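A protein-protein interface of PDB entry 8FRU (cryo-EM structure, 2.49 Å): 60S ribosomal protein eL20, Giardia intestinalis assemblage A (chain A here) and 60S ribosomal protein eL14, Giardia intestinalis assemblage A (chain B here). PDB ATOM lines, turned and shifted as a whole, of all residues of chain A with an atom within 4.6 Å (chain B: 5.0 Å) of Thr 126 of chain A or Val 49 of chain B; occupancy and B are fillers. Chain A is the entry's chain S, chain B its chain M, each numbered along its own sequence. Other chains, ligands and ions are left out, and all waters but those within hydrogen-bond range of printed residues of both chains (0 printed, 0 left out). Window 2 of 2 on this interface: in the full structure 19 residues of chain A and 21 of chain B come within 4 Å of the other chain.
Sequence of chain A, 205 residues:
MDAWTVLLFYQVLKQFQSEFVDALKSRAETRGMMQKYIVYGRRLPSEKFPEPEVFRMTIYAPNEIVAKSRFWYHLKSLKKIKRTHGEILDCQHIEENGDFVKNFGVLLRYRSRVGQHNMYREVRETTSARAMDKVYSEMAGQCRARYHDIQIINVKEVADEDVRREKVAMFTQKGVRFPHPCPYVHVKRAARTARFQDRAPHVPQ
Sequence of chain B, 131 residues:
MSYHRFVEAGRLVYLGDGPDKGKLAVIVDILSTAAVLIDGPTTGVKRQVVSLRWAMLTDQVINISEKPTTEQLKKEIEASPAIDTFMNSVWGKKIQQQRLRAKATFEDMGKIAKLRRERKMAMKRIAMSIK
The backbone NH of Lys 102 of chain A sits at hydrogen-bond distance from the backbone carbonyl oxygen of Glu 125 of chain A, at 2.8 Å. NH1 of Arg 130 of chain A lies within salt-bridge range of OE2 of Glu 125 of chain A, 3.1 Å away.
Glu 125 of chain A touches Leu 31 of chain B. CG2 of Thr 126 of chain A touches CG2 of Val 49 of chain B, 3.7 Å away. CG1 of Val 49 of chain B touches NH1 of Arg 130 of chain A, 3.98 Å away.
Of the printed residues of chain B, Arg 130 of chain A touches Val 49. Of the printed residues of chain A, Leu 31 of chain B touches Glu 125. Leu 37 of chain B touches none of the printed residues of chain A. Arg 47 of chain B touches none of the printed residues of chain A. Val 49 of chain B touches just these residues of chain A: Thr 126 and Arg 130. The nearest printed residue of chain B that does not touch Glu 125 of chain A is Val 49 of chain B (4.6 Å).
Hydrophobic or aromatic side chains of chain B within 4 Å of the printed part of chain A: Leu 31 and Val 49. Along chain B the printed residues that touch a printed residue of chain A span positions 31 to 49. Among the printed residues, 3 pairs touch across the chains. Among the printed residues, no Asp or Glu carboxylate lies within 4 Å of a Lys or Arg side-chain nitrogen of the other chain.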
ATOM      1  N   GLY A  98      11.118 -18.059 -21.632  1.00  0.00           N
ATOM      2  CA  GLY A  98      12.148 -18.984 -22.059  1.00  0.00           C
ATOM      3  C   GLY A  98      13.028 -18.486 -23.187  1.00  0.00           C
ATOM      4  O   GLY A  98      13.072 -19.096 -24.258  1.00  0.00           O
ATOM      5  N   PHE A 100      16.369 -16.362 -22.222  1.00  0.00           N
ATOM      6  CA  PHE A 100      17.701 -16.288 -21.644  1.00  0.00           C
ATOM      7  C   PHE A 100      17.893 -17.410 -20.634  1.00  0.00           C
ATOM      8  O   PHE A 100      16.988 -18.200 -20.366  1.00  0.00           O
ATOM      9  CB  PHE A 100      17.933 -14.919 -21.007  1.00  0.00           C
ATOM     10  CG  PHE A 100      17.601 -13.774 -21.909  1.00  0.00           C
ATOM     11  CD1 PHE A 100      18.469 -13.398 -22.914  1.00  0.00           C
ATOM     12  CD2 PHE A 100      16.418 -13.077 -21.760  1.00  0.00           C
ATOM     13  CE1 PHE A 100      18.168 -12.348 -23.746  1.00  0.00           C
ATOM     14  CE2 PHE A 100      16.112 -12.026 -22.592  1.00  0.00           C
ATOM     15  CZ  PHE A 100      16.988 -11.661 -23.584  1.00  0.00           C
ATOM     16  N   VAL A 101      19.097 -17.473 -20.073  1.00  0.00           N
ATOM     17  CA  VAL A 101      19.482 -18.512 -19.128  1.00  0.00           C
ATOM     18  C   VAL A 101      19.596 -17.886 -17.748  1.00  0.00           C
ATOM     19  O   VAL A 101      20.210 -16.824 -17.591  1.00  0.00           O
ATOM     20  CB  VAL A 101      20.803 -19.185 -19.533  1.00  0.00           C
ATOM     21  CG1 VAL A 101      21.317 -20.047 -18.405  1.00  0.00           C
ATOM     22  CG2 VAL A 101      20.613 -20.013 -20.784  1.00  0.00           C
ATOM     23  N   LYS A 102      19.009 -18.543 -16.752  1.00  0.00           N
ATOM     24  CA  LYS A 102      19.035 -18.066 -15.380  1.00  0.00           C
ATOM     25  C   LYS A 102      19.511 -19.182 -14.463  1.00  0.00           C
ATOM     26  O   LYS A 102      19.516 -20.358 -14.832  1.00  0.00           O
ATOM     27  CB  LYS A 102      17.656 -17.576 -14.933  1.00  0.00           C
ATOM     28  CG  LYS A 102      16.974 -16.682 -15.942  1.00  0.00           C
ATOM     29  CD  LYS A 102      15.486 -16.614 -15.687  1.00  0.00           C
ATOM     30  CE  LYS A 102      14.757 -15.981 -16.851  1.00  0.00           C
ATOM     31  NZ  LYS A 102      13.312 -15.790 -16.557  1.00  0.00           N
ATOM     32  N   GLU A 125      19.070 -23.055 -16.221  1.00  0.00           N
ATOM     33  CA  GLU A 125      18.006 -23.390 -17.157  1.00  0.00           C
ATOM     34  C   GLU A 125      17.373 -22.109 -17.680  1.00  0.00           C
ATOM     35  O   GLU A 125      17.692 -21.008 -17.234  1.00  0.00           O
ATOM     36  CB  GLU A 125      16.961 -24.288 -16.492  1.00  0.00           C
ATOM     37  CG  GLU A 125      16.113 -25.105 -17.445  1.00  0.00           C
ATOM     38  CD  GLU A 125      16.917 -26.057 -18.296  1.00  0.00           C
ATOM     39  OE1 GLU A 125      17.745 -26.803 -17.734  1.00  0.00           O
ATOM     40  OE2 GLU A 125      16.711 -26.069 -19.529  1.00  0.00           O
ATOM     41  N   THR A 126      16.470 -22.271 -18.644  1.00  0.00           N
ATOM     42  CA  THR A 126      15.754 -21.146 -19.228  1.00  0.00           C
ATOM     43  C   THR A 126      14.399 -20.891 -18.586  1.00  0.00           C
ATOM     44  O   THR A 126      13.881 -19.776 -18.695  1.00  0.00           O
ATOM     45  CB  THR A 126      15.559 -21.360 -20.734  1.00  0.00           C
ATOM     46  OG1 THR A 126      14.629 -22.426 -20.953  1.00  0.00           O
ATOM     47  CG2 THR A 126      16.878 -21.689 -21.407  1.00  0.00           C
ATOM     48  N   THR A 127      13.820 -21.884 -17.919  1.00  0.00           N
ATOM     49  CA  THR A 127      12.522 -21.745 -17.280  1.00  0.00           C
ATOM     50  C   THR A 127      12.540 -22.507 -15.965  1.00  0.00           C
ATOM     51  O   THR A 127      13.313 -23.450 -15.793  1.00  0.00           O
ATOM     52  CB  THR A 127      11.395 -22.271 -18.179  1.00  0.00           C
ATOM     53  OG1 THR A 127      11.280 -21.444 -19.341  1.00  0.00           O
ATOM     54  CG2 THR A 127      10.078 -22.272 -17.448  1.00  0.00           C
ATOM     55  N   ARG A 130      11.492 -26.078 -16.530  1.00  0.00           N
ATOM     56  CA  ARG A 130      12.565 -26.911 -17.055  1.00  0.00           C
ATOM     57  C   ARG A 130      13.608 -27.226 -15.993  1.00  0.00           C
ATOM     58  O   ARG A 130      14.275 -28.261 -16.072  1.00  0.00           O
ATOM     59  CB  ARG A 130      13.218 -26.223 -18.247  1.00  0.00           C
ATOM     60  CG  ARG A 130      12.424 -26.322 -19.525  1.00  0.00           C
ATOM     61  CD  ARG A 130      13.296 -26.005 -20.714  1.00  0.00           C
ATOM     62  NE  ARG A 130      13.109 -26.964 -21.793  1.00  0.00           N
ATOM     63  CZ  ARG A 130      14.047 -27.793 -22.229  1.00  0.00           C
ATOM     64  NH1 ARG A 130      15.255 -27.814 -21.692  1.00  0.00           N
ATOM     65  NH2 ARG A 130      13.765 -28.622 -23.228  1.00  0.00           N
ATOM     66  N   LEU B  31      24.564 -23.721 -21.149  1.00  0.00           N
ATOM     67  CA  LEU B  31      23.930 -24.098 -19.892  1.00  0.00           C
ATOM     68  C   LEU B  31      24.861 -24.928 -19.017  1.00  0.00           C
ATOM     69  O   LEU B  31      25.011 -24.655 -17.826  1.00  0.00           O
ATOM     70  CB  LEU B  31      22.642 -24.875 -20.166  1.00  0.00           C
ATOM     71  CG  LEU B  31      21.437 -24.050 -20.607  1.00  0.00           C
ATOM     72  CD1 LEU B  31      21.484 -23.823 -22.099  1.00  0.00           C
ATOM     73  CD2 LEU B  31      20.152 -24.742 -20.218  1.00  0.00           C
ATOM     74  N   ALA B  35      24.373 -29.166 -22.427  1.00  0.00           N
ATOM     75  CA  ALA B  35      23.348 -28.506 -23.219  1.00  0.00           C
ATOM     76  C   ALA B  35      23.757 -27.074 -23.525  1.00  0.00           C
ATOM     77  O   ALA B  35      24.505 -26.451 -22.771  1.00  0.00           O
ATOM     78  CB  ALA B  35      21.996 -28.520 -22.504  1.00  0.00           C
ATOM     79  N   VAL B  36      23.253 -26.563 -24.649  1.00  0.00           N
ATOM     80  CA  VAL B  36      23.507 -25.199 -25.093  1.00  0.00           C
ATOM     81  C   VAL B  36      22.209 -24.603 -25.613  1.00  0.00           C
ATOM     82  O   VAL B  36      21.251 -25.311 -25.919  1.00  0.00           O
ATOM     83  CB  VAL B  36      24.592 -25.123 -26.189  1.00  0.00           C
ATOM     84  CG1 VAL B  36      25.927 -25.574 -25.645  1.00  0.00           C
ATOM     85  CG2 VAL B  36      24.192 -25.951 -27.389  1.00  0.00           C
ATOM     86  N   LEU B  37      22.191 -23.280 -25.721  1.00  0.00           N
ATOM     87  CA  LEU B  37      21.057 -22.545 -26.263  1.00  0.00           C
ATOM     88  C   LEU B  37      21.430 -22.044 -27.648  1.00  0.00           C
ATOM     89  O   LEU B  37      22.332 -21.216 -27.785  1.00  0.00           O
ATOM     90  CB  LEU B  37      20.669 -21.386 -25.348  1.00  0.00           C
ATOM     91  CG  LEU B  37      19.424 -20.586 -25.720  1.00  0.00           C
ATOM     92  CD1 LEU B  37      18.186 -21.443 -25.607  1.00  0.00           C
ATOM     93  CD2 LEU B  37      19.307 -19.373 -24.827  1.00  0.00           C
ATOM     94  N   ARG B  47      14.694 -20.533 -31.673  1.00  0.00           N
ATOM     95  CA  ARG B  47      15.488 -20.533 -30.453  1.00  0.00           C
ATOM     96  C   ARG B  47      15.043 -21.670 -29.539  1.00  0.00           C
ATOM     97  O   ARG B  47      13.847 -21.846 -29.294  1.00  0.00           O
ATOM     98  CB  ARG B  47      15.355 -19.188 -29.748  1.00  0.00           C
ATOM     99  CG  ARG B  47      16.546 -18.801 -28.906  1.00  0.00           C
ATOM    100  CD  ARG B  47      16.133 -17.817 -27.840  1.00  0.00           C
ATOM    101  NE  ARG B  47      17.234 -16.987 -27.376  1.00  0.00           N
ATOM    102  CZ  ARG B  47      17.790 -16.010 -28.079  1.00  0.00           C
ATOM    103  NH1 ARG B  47      17.404 -15.740 -29.312  1.00  0.00           N
ATOM    104  NH2 ARG B  47      18.762 -15.291 -27.530  1.00  0.00           N
ATOM    105  N   GLN B  48      15.999 -22.445 -29.037  1.00  0.00           N
ATOM    106  CA  GLN B  48      15.673 -23.599 -28.208  1.00  0.00           C
ATOM    107  C   GLN B  48      16.945 -24.132 -27.565  1.00  0.00           C
ATOM    108  O   GLN B  48      18.055 -23.716 -27.894  1.00  0.00           O
ATOM    109  CB  GLN B  48      14.990 -24.698 -29.020  1.00  0.00           C
ATOM    110  CG  GLN B  48      15.906 -25.365 -30.015  1.00  0.00           C
ATOM    111  CD  GLN B  48      15.166 -25.915 -31.203  1.00  0.00           C
ATOM    112  OE1 GLN B  48      14.580 -26.991 -31.141  1.00  0.00           O
ATOM    113  NE2 GLN B  48      15.176 -25.172 -32.297  1.00  0.00           N
ATOM    114  N   VAL B  49      16.761 -25.077 -26.650  1.00  0.00           N
ATOM    115  CA  VAL B  49      17.851 -25.718 -25.925  1.00  0.00           C
ATOM    116  C   VAL B  49      18.009 -27.137 -26.449  1.00  0.00           C
ATOM    117  O   VAL B  49      17.029 -27.883 -26.538  1.00  0.00           O
ATOM    118  CB  VAL B  49      17.589 -25.721 -24.411  1.00  0.00           C
ATOM    119  CG1 VAL B  49      18.496 -26.716 -23.717  1.00  0.00           C
ATOM    120  CG2 VAL B  49      17.775 -24.331 -23.844  1.00  0.00           C
ATOM    121  N   VAL B  50      19.239 -27.511 -26.799  1.00  0.00           N
ATOM    122  CA  VAL B  50      19.538 -28.851 -27.282  1.00  0.00           C
ATOM    123  C   VAL B  50      20.735 -29.392 -26.519  1.00  0.00           C
ATOM    124  O   VAL B  50      21.507 -28.647 -25.914  1.00  0.00           O
ATOM    125  CB  VAL B  50      19.819 -28.889 -28.799  1.00  0.00           C
ATOM    126  CG1 VAL B  50      18.603 -28.438 -29.579  1.00  0.00           C
ATOM    127  CG2 VAL B  50      21.022 -28.038 -29.133  1.00  0.00           C
ATOM    128  N   SER B  51      20.884 -30.710 -26.552  1.00  0.00           N
ATOM    129  CA  SER B  51      22.051 -31.351 -25.973  1.00  0.00           C
ATOM    130  C   SER B  51      23.191 -31.360 -26.981  1.00  0.00           C
ATOM    131  O   SER B  51      22.977 -31.451 -28.189  1.00  0.00           O
ATOM    132  CB  SER B  51      21.729 -32.776 -25.518  1.00  0.00           C
ATOM    133  OG  SER B  51      21.838 -33.707 -26.574  1.00  0.00           O
